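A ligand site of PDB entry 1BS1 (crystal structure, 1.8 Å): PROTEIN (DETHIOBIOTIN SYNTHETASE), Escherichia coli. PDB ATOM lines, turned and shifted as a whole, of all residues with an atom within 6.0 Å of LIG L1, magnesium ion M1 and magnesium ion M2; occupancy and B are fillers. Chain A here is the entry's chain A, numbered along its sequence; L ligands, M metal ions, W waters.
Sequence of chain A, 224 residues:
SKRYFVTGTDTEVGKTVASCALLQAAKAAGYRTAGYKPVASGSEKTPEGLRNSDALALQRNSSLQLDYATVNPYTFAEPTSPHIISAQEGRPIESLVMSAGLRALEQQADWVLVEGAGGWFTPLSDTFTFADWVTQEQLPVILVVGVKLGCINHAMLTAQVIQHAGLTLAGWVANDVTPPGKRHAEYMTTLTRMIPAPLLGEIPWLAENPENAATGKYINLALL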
ATOM      1  N   GLY A   8     -23.410  -7.864 -16.162  1.00  0.00           N
ATOM      2  CA  GLY A   8     -23.872  -6.473 -16.246  1.00  0.00           C
ATOM      3  C   GLY A   8     -23.686  -5.895 -17.654  1.00  0.00           C
ATOM      4  O   GLY A   8     -22.981  -6.408 -18.514  1.00  0.00           O
ATOM      5  N   ASP A  10     -22.030  -3.409 -18.319  1.00  0.00           N
ATOM      6  CA  ASP A  10     -20.684  -2.831 -18.410  1.00  0.00           C
ATOM      7  C   ASP A  10     -20.029  -3.055 -17.033  1.00  0.00           C
ATOM      8  O   ASP A  10     -20.655  -3.678 -16.182  1.00  0.00           O
ATOM      9  CB  ASP A  10     -20.737  -1.341 -18.707  1.00  0.00           C
ATOM     10  CG  ASP A  10     -19.458  -0.651 -19.134  1.00  0.00           C
ATOM     11  OD1 ASP A  10     -18.407  -1.281 -19.254  1.00  0.00           O
ATOM     12  OD2 ASP A  10     -19.486   0.573 -19.395  1.00  0.00           O
ATOM     13  N   THR A  11     -18.796  -2.582 -16.869  1.00  0.00           N
ATOM     14  CA  THR A  11     -18.215  -2.583 -15.515  1.00  0.00           C
ATOM     15  C   THR A  11     -18.808  -1.334 -14.860  1.00  0.00           C
ATOM     16  O   THR A  11     -19.268  -0.439 -15.608  1.00  0.00           O
ATOM     17  CB  THR A  11     -16.684  -2.543 -15.573  1.00  0.00           C
ATOM     18  OG1 THR A  11     -16.093  -2.748 -14.262  1.00  0.00           O
ATOM     19  CG2 THR A  11     -16.188  -1.230 -16.178  1.00  0.00           C
ATOM     20  N   GLU A  12     -18.863  -1.262 -13.545  1.00  0.00           N
ATOM     21  CA  GLU A  12     -19.349  -0.095 -12.827  1.00  0.00           C
ATOM     22  C   GLU A  12     -20.796   0.284 -13.072  1.00  0.00           C
ATOM     23  O   GLU A  12     -21.140   1.479 -13.157  1.00  0.00           O
ATOM     24  CB  GLU A  12     -18.402   1.086 -13.150  1.00  0.00           C
ATOM     25  CG  GLU A  12     -17.998   1.921 -11.963  1.00  0.00           C
ATOM     26  CD  GLU A  12     -17.303   1.233 -10.815  1.00  0.00           C
ATOM     27  OE1 GLU A  12     -16.615   0.194 -10.919  1.00  0.00           O
ATOM     28  OE2 GLU A  12     -17.410   1.740  -9.670  1.00  0.00           O
ATOM     29  N   VAL A  13     -21.684  -0.713 -13.122  1.00  0.00           N
ATOM     30  CA  VAL A  13     -23.114  -0.462 -13.304  1.00  0.00           C
ATOM     31  C   VAL A  13     -23.950  -0.952 -12.128  1.00  0.00           C
ATOM     32  O   VAL A  13     -25.157  -0.752 -12.117  1.00  0.00           O
ATOM     33  CB  VAL A  13     -23.668  -1.073 -14.605  1.00  0.00           C
ATOM     34  CG1 VAL A  13     -22.935  -0.498 -15.815  1.00  0.00           C
ATOM     35  CG2 VAL A  13     -23.575  -2.598 -14.598  1.00  0.00           C
ATOM     36  N   GLY A  14     -23.357  -1.633 -11.153  1.00  0.00           N
ATOM     37  CA  GLY A  14     -24.063  -2.200 -10.004  1.00  0.00           C
ATOM     38  C   GLY A  14     -24.161  -3.699  -9.887  1.00  0.00           C
ATOM     39  O   GLY A  14     -24.997  -4.195  -9.110  1.00  0.00           O
ATOM     40  N   LYS A  15     -23.389  -4.495 -10.618  1.00  0.00           N
ATOM     41  CA  LYS A  15     -23.440  -5.945 -10.450  1.00  0.00           C
ATOM     42  C   LYS A  15     -23.271  -6.326  -8.974  1.00  0.00           C
ATOM     43  O   LYS A  15     -24.016  -7.174  -8.465  1.00  0.00           O
ATOM     44  CB  LYS A  15     -22.375  -6.742 -11.218  1.00  0.00           C
ATOM     45  CG  LYS A  15     -22.459  -6.640 -12.740  1.00  0.00           C
ATOM     46  CD  LYS A  15     -21.459  -7.564 -13.406  1.00  0.00           C
ATOM     47  CE  LYS A  15     -20.013  -7.238 -13.018  1.00  0.00           C
ATOM     48  NZ  LYS A  15     -19.616  -5.924 -13.648  1.00  0.00           N
ATOM     49  N   THR A  16     -22.234  -5.767  -8.335  1.00  0.00           N
ATOM     50  CA  THR A  16     -21.994  -6.130  -6.918  1.00  0.00           C
ATOM     51  C   THR A  16     -23.148  -5.714  -6.023  1.00  0.00           C
ATOM     52  O   THR A  16     -23.589  -6.526  -5.198  1.00  0.00           O
ATOM     53  CB  THR A  16     -20.654  -5.523  -6.460  1.00  0.00           C
ATOM     54  OG1 THR A  16     -19.635  -6.116  -7.308  1.00  0.00           O
ATOM     55  CG2 THR A  16     -20.352  -5.908  -5.006  1.00  0.00           C
ATOM     56  N   VAL A  17     -23.602  -4.457  -6.158  1.00  0.00           N
ATOM     57  CA  VAL A  17     -24.706  -4.008  -5.299  1.00  0.00           C
ATOM     58  C   VAL A  17     -25.931  -4.881  -5.551  1.00  0.00           C
ATOM     59  O   VAL A  17     -26.593  -5.333  -4.618  1.00  0.00           O
ATOM     60  CB  VAL A  17     -25.003  -2.515  -5.552  1.00  0.00           C
ATOM     61  CG1 VAL A  17     -26.371  -2.114  -5.065  1.00  0.00           C
ATOM     62  CG2 VAL A  17     -23.925  -1.660  -4.881  1.00  0.00           C
ATOM     63  N   ALA A  18     -26.261  -5.138  -6.811  1.00  0.00           N
ATOM     64  CA  ALA A  18     -27.408  -5.992  -7.111  1.00  0.00           C
ATOM     65  C   ALA A  18     -27.191  -7.428  -6.631  1.00  0.00           C
ATOM     66  O   ALA A  18     -28.149  -8.060  -6.158  1.00  0.00           O
ATOM     67  CB  ALA A  18     -27.703  -5.896  -8.612  1.00  0.00           C
ATOM     68  N   LYS A  37     -17.180 -15.006  -6.478  1.00  0.00           N
ATOM     69  CA  LYS A  37     -16.538 -14.088  -7.442  1.00  0.00           C
ATOM     70  C   LYS A  37     -15.242 -14.819  -7.791  1.00  0.00           C
ATOM     71  O   LYS A  37     -14.177 -14.556  -7.201  1.00  0.00           O
ATOM     72  CB  LYS A  37     -16.218 -12.760  -6.755  1.00  0.00           C
ATOM     73  CG  LYS A  37     -15.440 -11.747  -7.598  1.00  0.00           C
ATOM     74  CD  LYS A  37     -16.361 -10.815  -8.385  1.00  0.00           C
ATOM     75  CE  LYS A  37     -15.555  -9.747  -9.123  1.00  0.00           C
ATOM     76  NZ  LYS A  37     -16.366  -8.827  -9.984  1.00  0.00           N
ATOM     77  N   ASP A  54     -15.470  -6.590  -4.119  1.00  0.00           N
ATOM     78  CA  ASP A  54     -16.691  -7.300  -4.511  1.00  0.00           C
ATOM     79  C   ASP A  54     -16.767  -8.623  -3.741  1.00  0.00           C
ATOM     80  O   ASP A  54     -17.797  -9.015  -3.192  1.00  0.00           O
ATOM     81  CB  ASP A  54     -16.664  -7.620  -6.019  1.00  0.00           C
ATOM     82  CG  ASP A  54     -16.700  -6.441  -6.978  1.00  0.00           C
ATOM     83  OD1 ASP A  54     -16.659  -5.282  -6.524  1.00  0.00           O
ATOM     84  OD2 ASP A  54     -16.760  -6.659  -8.228  1.00  0.00           O
ATOM     85  N   GLU A 115     -20.826 -13.867  -9.332  1.00  0.00           N
ATOM     86  CA  GLU A 115     -20.698 -12.542  -9.969  1.00  0.00           C
ATOM     87  C   GLU A 115     -19.551 -12.586 -10.984  1.00  0.00           C
ATOM     88  O   GLU A 115     -18.486 -13.098 -10.654  1.00  0.00           O
ATOM     89  CB  GLU A 115     -20.477 -11.406  -8.969  1.00  0.00           C
ATOM     90  CG  GLU A 115     -20.366 -10.054  -9.688  1.00  0.00           C
ATOM     91  CD  GLU A 115     -19.917  -8.894  -8.813  1.00  0.00           C
ATOM     92  OE1 GLU A 115     -19.901  -9.035  -7.577  1.00  0.00           O
ATOM     93  OE2 GLU A 115     -19.592  -7.860  -9.446  1.00  0.00           O
ATOM     94  N   GLY A 116     -19.791 -12.067 -12.193  1.00  0.00           N
ATOM     95  CA  GLY A 116     -18.755 -12.067 -13.232  1.00  0.00           C
ATOM     96  C   GLY A 116     -17.787 -10.908 -13.018  1.00  0.00           C
ATOM     97  O   GLY A 116     -17.822 -10.320 -11.933  1.00  0.00           O
ATOM     98  N   GLY A 118     -16.462  -7.386 -14.958  1.00  0.00           N
ATOM     99  CA  GLY A 118     -16.741  -6.528 -16.118  1.00  0.00           C
ATOM    100  C   GLY A 118     -18.053  -6.990 -16.756  1.00  0.00           C
ATOM    101  O   GLY A 118     -18.970  -7.403 -16.038  1.00  0.00           O
ATOM    102  N   ASN A 175     -30.778  -1.099 -11.840  1.00  0.00           N
ATOM    103  CA  ASN A 175     -30.053  -0.468 -10.740  1.00  0.00           C
ATOM    104  C   ASN A 175     -29.904   1.032 -11.008  1.00  0.00           C
ATOM    105  O   ASN A 175     -29.405   1.481 -12.052  1.00  0.00           O
ATOM    106  CB  ASN A 175     -28.702  -1.147 -10.548  1.00  0.00           C
ATOM    107  CG  ASN A 175     -27.929  -0.508  -9.393  1.00  0.00           C
ATOM    108  OD1 ASN A 175     -28.483  -0.422  -8.316  1.00  0.00           O
ATOM    109  ND2 ASN A 175     -26.704  -0.088  -9.667  1.00  0.00           N
ATOM    110  N   ASP A 176     -30.453   1.828 -10.082  1.00  0.00           N
ATOM    111  CA  ASP A 176     -30.426   3.281 -10.208  1.00  0.00           C
ATOM    112  C   ASP A 176     -29.103   3.856  -9.714  1.00  0.00           C
ATOM    113  O   ASP A 176     -28.937   4.254  -8.550  1.00  0.00           O
ATOM    114  CB  ASP A 176     -31.595   3.889  -9.447  1.00  0.00           C
ATOM    115  CG  ASP A 176     -32.937   3.338  -9.841  1.00  0.00           C
ATOM    116  OD1 ASP A 176     -33.083   2.655 -10.885  1.00  0.00           O
ATOM    117  OD2 ASP A 176     -33.907   3.574  -9.090  1.00  0.00           O
ATOM    118  N   VAL A 177     -28.165   3.935 -10.637  1.00  0.00           N
ATOM    119  CA  VAL A 177     -26.814   4.388 -10.362  1.00  0.00           C
ATOM    120  C   VAL A 177     -26.679   5.875 -10.071  1.00  0.00           C
ATOM    121  O   VAL A 177     -25.703   6.290  -9.417  1.00  0.00           O
ATOM    122  CB  VAL A 177     -25.846   4.004 -11.511  1.00  0.00           C
ATOM    123  CG1 VAL A 177     -25.546   2.514 -11.370  1.00  0.00           C
ATOM    124  CG2 VAL A 177     -26.411   4.338 -12.889  1.00  0.00           C
ATOM    125  N   THR A 178     -27.642   6.664 -10.499  1.00  0.00           N
ATOM    126  CA  THR A 178     -27.647   8.094 -10.221  1.00  0.00           C
ATOM    127  C   THR A 178     -29.028   8.516  -9.739  1.00  0.00           C
ATOM    128  O   THR A 178     -29.992   7.788  -9.912  1.00  0.00           O
ATOM    129  CB  THR A 178     -27.361   8.939 -11.496  1.00  0.00           C
ATOM    130  OG1 THR A 178     -28.386   8.708 -12.471  1.00  0.00           O
ATOM    131  CG2 THR A 178     -26.000   8.628 -12.069  1.00  0.00           C
ATOM    132  N   ILE A 203     -33.278  -1.395  -7.770  1.00  0.00           N
ATOM    133  CA  ILE A 203     -32.591  -0.905  -6.581  1.00  0.00           C
ATOM    134  C   ILE A 203     -32.485   0.608  -6.704  1.00  0.00           C
ATOM    135  O   ILE A 203     -32.032   1.077  -7.753  1.00  0.00           O
ATOM    136  CB  ILE A 203     -31.231  -1.575  -6.441  1.00  0.00           C
ATOM    137  CG1 ILE A 203     -31.488  -3.097  -6.214  1.00  0.00           C
ATOM    138  CG2 ILE A 203     -30.386  -1.020  -5.294  1.00  0.00           C
ATOM    139  CD1 ILE A 203     -30.234  -3.921  -6.415  1.00  0.00           C
ATOM    140  N   PRO A 204     -32.971   1.349  -5.715  1.00  0.00           N
ATOM    141  CA  PRO A 204     -32.971   2.798  -5.804  1.00  0.00           C
ATOM    142  C   PRO A 204     -31.576   3.380  -5.604  1.00  0.00           C
ATOM    143  O   PRO A 204     -30.672   2.654  -5.235  1.00  0.00           O
ATOM    144  CB  PRO A 204     -33.862   3.230  -4.634  1.00  0.00           C
ATOM    145  CG  PRO A 204     -33.953   2.057  -3.710  1.00  0.00           C
ATOM    146  CD  PRO A 204     -33.521   0.807  -4.447  1.00  0.00           C
ATOM    147  N   TRP A 205     -31.423   4.670  -5.903  1.00  0.00           N
ATOM    148  CA  TRP A 205     -30.140   5.347  -5.709  1.00  0.00           C
ATOM    149  C   TRP A 205     -29.884   5.492  -4.204  1.00  0.00           C
ATOM    150  O   TRP A 205     -30.589   6.185  -3.468  1.00  0.00           O
ATOM    151  CB  TRP A 205     -30.143   6.718  -6.416  1.00  0.00           C
ATOM    152  CG  TRP A 205     -28.898   7.521  -6.164  1.00  0.00           C
ATOM    153  CD1 TRP A 205     -27.652   7.238  -6.631  1.00  0.00           C
ATOM    154  CD2 TRP A 205     -28.792   8.734  -5.410  1.00  0.00           C
ATOM    155  NE1 TRP A 205     -26.774   8.210  -6.203  1.00  0.00           N
ATOM    156  CE2 TRP A 205     -27.445   9.133  -5.448  1.00  0.00           C
ATOM    157  CE3 TRP A 205     -29.697   9.516  -4.701  1.00  0.00           C
ATOM    158  CZ2 TRP A 205     -26.975  10.277  -4.810  1.00  0.00           C
ATOM    159  CZ3 TRP A 205     -29.241  10.658  -4.070  1.00  0.00           C
ATOM    160  CH2 TRP A 205     -27.891  11.027  -4.123  1.00  0.00           C
ATOM    161  N   LEU A 206     -28.845   4.802  -3.737  1.00  0.00           N
ATOM    162  CA  LEU A 206     -28.419   4.734  -2.357  1.00  0.00           C
ATOM    163  C   LEU A 206     -26.975   5.203  -2.237  1.00  0.00           C
ATOM    164  O   LEU A 206     -26.027   4.420  -2.290  1.00  0.00           O
ATOM    165  CB  LEU A 206     -28.543   3.300  -1.803  1.00  0.00           C
ATOM    166  CG  LEU A 206     -29.974   2.743  -1.752  1.00  0.00           C
ATOM    167  CD1 LEU A 206     -29.945   1.227  -1.834  1.00  0.00           C
ATOM    168  CD2 LEU A 206     -30.642   3.243  -0.484  1.00  0.00           C
ATOM    169  N   ALA A 207     -26.806   6.515  -2.129  1.00  0.00           N
ATOM    170  CA  ALA A 207     -25.502   7.157  -2.075  1.00  0.00           C
ATOM    171  C   ALA A 207     -24.491   6.511  -1.105  1.00  0.00           C
ATOM    172  O   ALA A 207     -23.369   6.160  -1.505  1.00  0.00           O
ATOM    173  CB  ALA A 207     -25.727   8.619  -1.753  1.00  0.00           C
ATOM    174  N   PRO A 210     -24.075   1.295  -0.371  1.00  0.00           N
ATOM    175  CA  PRO A 210     -25.207   0.534  -0.878  1.00  0.00           C
ATOM    176  C   PRO A 210     -25.018  -0.977  -0.760  1.00  0.00           C
ATOM    177  O   PRO A 210     -26.006  -1.729  -0.747  1.00  0.00           O
ATOM    178  CB  PRO A 210     -25.373   1.010  -2.328  1.00  0.00           C
ATOM    179  CG  PRO A 210     -24.074   1.621  -2.707  1.00  0.00           C
ATOM    180  CD  PRO A 210     -23.426   2.103  -1.436  1.00  0.00           C
ATOM    181  N   GLU A 211     -23.789  -1.432  -0.695  1.00  0.00           N
ATOM    182  CA  GLU A 211     -23.459  -2.846  -0.585  1.00  0.00           C
ATOM    183  C   GLU A 211     -23.951  -3.472   0.737  1.00  0.00           C
ATOM    184  O   GLU A 211     -24.235  -4.677   0.804  1.00  0.00           O
ATOM    185  CB  GLU A 211     -21.946  -3.063  -0.722  1.00  0.00           C
ATOM    186  CG  GLU A 211     -21.366  -2.708  -2.084  1.00  0.00           C
ATOM    187  CD  GLU A 211     -21.107  -1.228  -2.306  1.00  0.00           C
ATOM    188  OE1 GLU A 211     -21.158  -0.438  -1.332  1.00  0.00           O
ATOM    189  OE2 GLU A 211     -20.858  -0.806  -3.458  1.00  0.00           O
HETATM  190  P1  LIG L   1     -19.959  -3.363 -10.878  1.00  0.00           P
HETATM  191  O1  LIG L   1     -20.903  -3.517 -12.035  1.00  0.00           O
HETATM  192  O2  LIG L   1     -19.929  -4.539  -9.814  1.00  0.00           O
HETATM  193  O3  LIG L   1     -18.536  -3.028 -11.220  1.00  0.00           O
HETATM  194  P2  LIG L   1     -20.791  -1.920  -8.293  1.00  0.00           P
HETATM  195  O4  LIG L   1     -19.448  -2.092  -7.663  1.00  0.00           O
HETATM  196  O5  LIG L   1     -21.935  -2.685  -7.741  1.00  0.00           O
HETATM  197  O6  LIG L   1     -20.623  -2.149  -9.997  1.00  0.00           O
HETATM  198  O7  LIG L   1     -21.249  -0.311  -8.398  1.00  0.00           O
HETATM  199  C1  LIG L   1     -20.330   0.648  -9.058  1.00  0.00           C
HETATM  200  C2  LIG L   1     -20.231   1.889  -8.177  1.00  0.00           C
HETATM  201  O8  LIG L   1     -21.537   2.486  -8.153  1.00  0.00           O
HETATM  202  C3  LIG L   1     -19.873   1.612  -6.724  1.00  0.00           C
HETATM  203  O9  LIG L   1     -19.083   2.695  -6.158  1.00  0.00           O
HETATM  204  C4  LIG L   1     -21.180   1.495  -5.975  1.00  0.00           C
HETATM  205  O10 LIG L   1     -21.074   1.796  -4.560  1.00  0.00           O
HETATM  206  C5  LIG L   1     -22.016   2.506  -6.773  1.00  0.00           C
HETATM  207  N1  LIG L   1     -23.456   2.023  -6.696  1.00  0.00           N
HETATM  208  C6  LIG L   1     -23.915   0.979  -7.407  1.00  0.00           C
HETATM  209  N2  LIG L   1     -25.226   0.925  -7.279  1.00  0.00           N
HETATM  210  C7  LIG L   1     -25.642   1.996  -6.622  1.00  0.00           C
HETATM  211  C8  LIG L   1     -26.895   2.378  -6.148  1.00  0.00           C
HETATM  212  N3  LIG L   1     -28.009   1.686  -6.405  1.00  0.00           N
HETATM  213  N4  LIG L   1     -26.952   3.579  -5.528  1.00  0.00           N
HETATM  214  C9  LIG L   1     -25.869   4.351  -5.455  1.00  0.00           C
HETATM  215  N5  LIG L   1     -24.637   3.893  -5.619  1.00  0.00           N
HETATM  216  C10 LIG L   1     -24.523   2.768  -6.354  1.00  0.00           C
HETATM  217  C1  LG2 L   2     -12.780  -5.945 -19.770  1.00  0.00           C
HETATM  218  C2  LG2 L   2     -13.231  -5.007 -20.921  1.00  0.00           C
HETATM  219  O1  LG2 L   2     -12.505  -4.047 -21.238  1.00  0.00           O
HETATM  220  O2  LG2 L   2     -14.299  -5.273 -21.471  1.00  0.00           O
HETATM  221  C3  LG2 L   2     -13.007  -5.127 -18.465  1.00  0.00           C
HETATM  222  C4  LG2 L   2     -12.443  -5.774 -17.221  1.00  0.00           C
HETATM  223  C5  LG2 L   2     -13.151  -5.151 -15.995  1.00  0.00           C
HETATM  224  C6  LG2 L   2     -12.694  -5.991 -14.787  1.00  0.00           C
HETATM  225  C7  LG2 L   2     -13.294  -5.627 -13.416  1.00  0.00           C
HETATM  226  C8  LG2 L   2     -12.901  -4.168 -13.070  1.00  0.00           C
HETATM  227  C9  LG2 L   2     -11.376  -4.051 -13.143  1.00  0.00           C
HETATM  228  N1  LG2 L   2     -12.756  -6.565 -12.361  1.00  0.00           N
HETATM  229  C10 LG2 L   2     -13.657  -7.169 -11.509  1.00  0.00           C
HETATM  230  O3  LG2 L   2     -15.055  -7.069 -11.853  1.00  0.00           O
HETATM  231  O4  LG2 L   2     -13.331  -7.827 -10.490  1.00  0.00           O
HETATM  232  N2  LG2 L   2     -13.227  -4.107 -11.626  1.00  0.00           N
HETATM  233 AL1  LG2 L   2     -16.395  -5.765 -11.993  1.00  0.00          AL
HETATM  234  F1  LG2 L   2     -17.545  -6.050 -10.928  1.00  0.00           F
HETATM  235  F2  LG2 L   2     -15.527  -4.526 -11.451  1.00  0.00           F
HETATM  236  F3  LG2 L   2     -17.141  -5.176 -13.317  1.00  0.00           F
HETATM  237 MG    MG M   1     -18.642  -5.854  -9.153  1.00  0.00          MG
HETATM  238 MG    MG M   2     -16.622  -2.929 -10.161  1.00  0.00          MG
HETATM  239  O   HOH W   1     -19.099  -1.908  -5.067  1.00  0.00           O
HETATM  240  O   HOH W   2     -22.559   5.427  -4.441  1.00  0.00           O
HETATM  241  O   HOH W   3     -19.835   1.754  -1.568  1.00  0.00           O
HETATM  242  O   HOH W   4     -21.362   5.724  -8.816  1.00  0.00           O
HETATM  243  O   HOH W   5     -14.411  -2.465  -9.325  1.00  0.00           O
HETATM  244  O   HOH W   6     -20.386   4.406  -3.572  1.00  0.00           O
HETATM  245  O   HOH W   7     -16.889   2.873  -7.513  1.00  0.00           O
HETATM  246  O   HOH W   8     -17.100  -0.922  -8.015  1.00  0.00           O
HETATM  247  O   HOH W   9     -17.644  -3.761  -8.383  1.00  0.00           O
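NZ of Lys 15 is in salt-bridge range of O1 of LIG L1.
An oxygen (O1) of LIG L1 sits at hydrogen-bond distance from the backbone NH (N) of Glu 12 (3.4 Å).
The side-chain amino group (NZ) of Lys 15 lies within hydrogen-bond range of a fluorine (F3) of LG2 L2, at 2.6 Å.
An oxygen (O5) of LIG L1 sits at hydrogen-bond distance from the backbone NH (N) of Thr 16, at 3.2 Å.
The backbone NH of Lys 15 sits at hydrogen-bond distance from an oxygen (O1) of LIG L1, at 3.0 Å.
N of Leu 206 is in hydrogen-bond range of N4 of LIG L1 (2.9 Å).
The backbone carbonyl oxygen of Pro 204 lies within hydrogen-bond range of a nitrogen (N3) of LIG L1 (3.1 Å).
A nitrogen (N3) of LIG L1 sits at hydrogen-bond distance from the side-chain amide oxygen (OD1) of Asn 175, 2.9 Å away.
The side-chain amino group of Lys 37 lies within salt-bridge range of an oxygen (O4) of LG2 L2.
A fluorine (F3) of LG2 L2 lies within hydrogen-bond range of the backbone NH (N) of Gly 118.
The backbone NH (N) of Val 13 is in hydrogen-bond range of an oxygen (O1) of LIG L1, 3.1 Å away.
O of Asp 176 is in hydrogen-bond range of N3 of LIG L1, 3.5 Å away.
O5 of LIG L1 lies within hydrogen-bond range of N of Val 17 (2.9 Å).
The backbone NH (N) of Gly 14 sits at hydrogen-bond distance from an oxygen (O6) of LIG L1, 3.0 Å away.
OG1 of Thr 11 is in hydrogen-bond range of F3 of LG2 L2.
The side-chain carboxylate (OE2) of Glu 211 sits at hydrogen-bond distance from an oxygen (O10) of LIG L1, at 2.8 Å.
The side-chain amide nitrogen (ND2) of Asn 175 sits at hydrogen-bond distance from the backbone carbonyl oxygen (O) of Val 13, 3.0 Å away.
The side-chain carboxylate of Glu 115 lies close to the side-chain amino group of Lys 37.
N of Asp 176 lies within hydrogen-bond range of O of Ile 203 (2.9 Å).
NZ of Lys 37 lies within hydrogen-bond range of O of Gly 116, at 2.9 Å.
The side-chain carboxylate (OD2) of Asp 54 lies close to the side-chain amino group (NZ) of Lys 37 (2.8 Å).
NZ of Lys 15 sits at hydrogen-bond distance from O of Gly 118, 2.9 Å away.
OG1 of Thr 11 touches O3 of LIG L1 (3.9 Å).
CG2 of Ile 203 touches N3 of LIG L1 (3.8 Å).
Trp 205 touches LIG L1 (CD1 to C9, 3.6 Å).
Pro 210 touches LIG L1.
Hydrophobic or aromatic side chains that line LIG L1: Val 13, Val 17, Ile 203, Trp 205 and Pro 210.
Of the 26 residues printed, 16 come within 4 Å of LIG L1.
Merely in contact with magnesium ion M1: Lys 37.
Within 4 Å of magnesium ion M1: Thr 16, Lys 37, Asp 54 and Glu 115.
The nearest printed residue that does not touch magnesium ion M1 is Lys 15 (4.3 Å).
Residues that only touch magnesium ion M2: Glu 12 (3.2 Å).
Magnesium ion M1 is bound by O2 of LIG L1, F1 of LG2 L2, OG1 of Thr 16, OE2 of Glu 115, OD2 of Asp 54 and water W9.
An oxygen (O3) of LIG L1 is bound to magnesium ion M2 (2.2 Å).
Water W9 binds magnesium ion M2 (2.2 Å).
Magnesium ion M2 is bound by F2 of LG2 L2, at 2.3 Å.
Water W5 binds magnesium ion M2, 2.4 Å away.
Water W9 bridges O4 of LIG L1 (2.6 Å) and OD1 of Asp 54 (2.6 Å).
Water W7 bridges the side-chain carboxylate (OE2) of Glu 12 and an oxygen (O9) of LIG L1.
Water W1 lies within hydrogen-bond range of the side-chain carboxylate of Glu 211 (2.6 Å) and an oxygen (O4) of LIG L1 (2.6 Å).
Water W8 lies within hydrogen-bond range of O4 of LIG L1 (2.6 Å) and OE1 of Glu 12 (3.1 Å).
Water W2 lies within hydrogen-bond range of a nitrogen (N5) of LIG L1 and the backbone carbonyl oxygen of Ala 207.
Water W3 lies within hydrogen-bond range of OE1 of Glu 211 (2.6 Å) and O10 of LIG L1 (3.2 Å).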
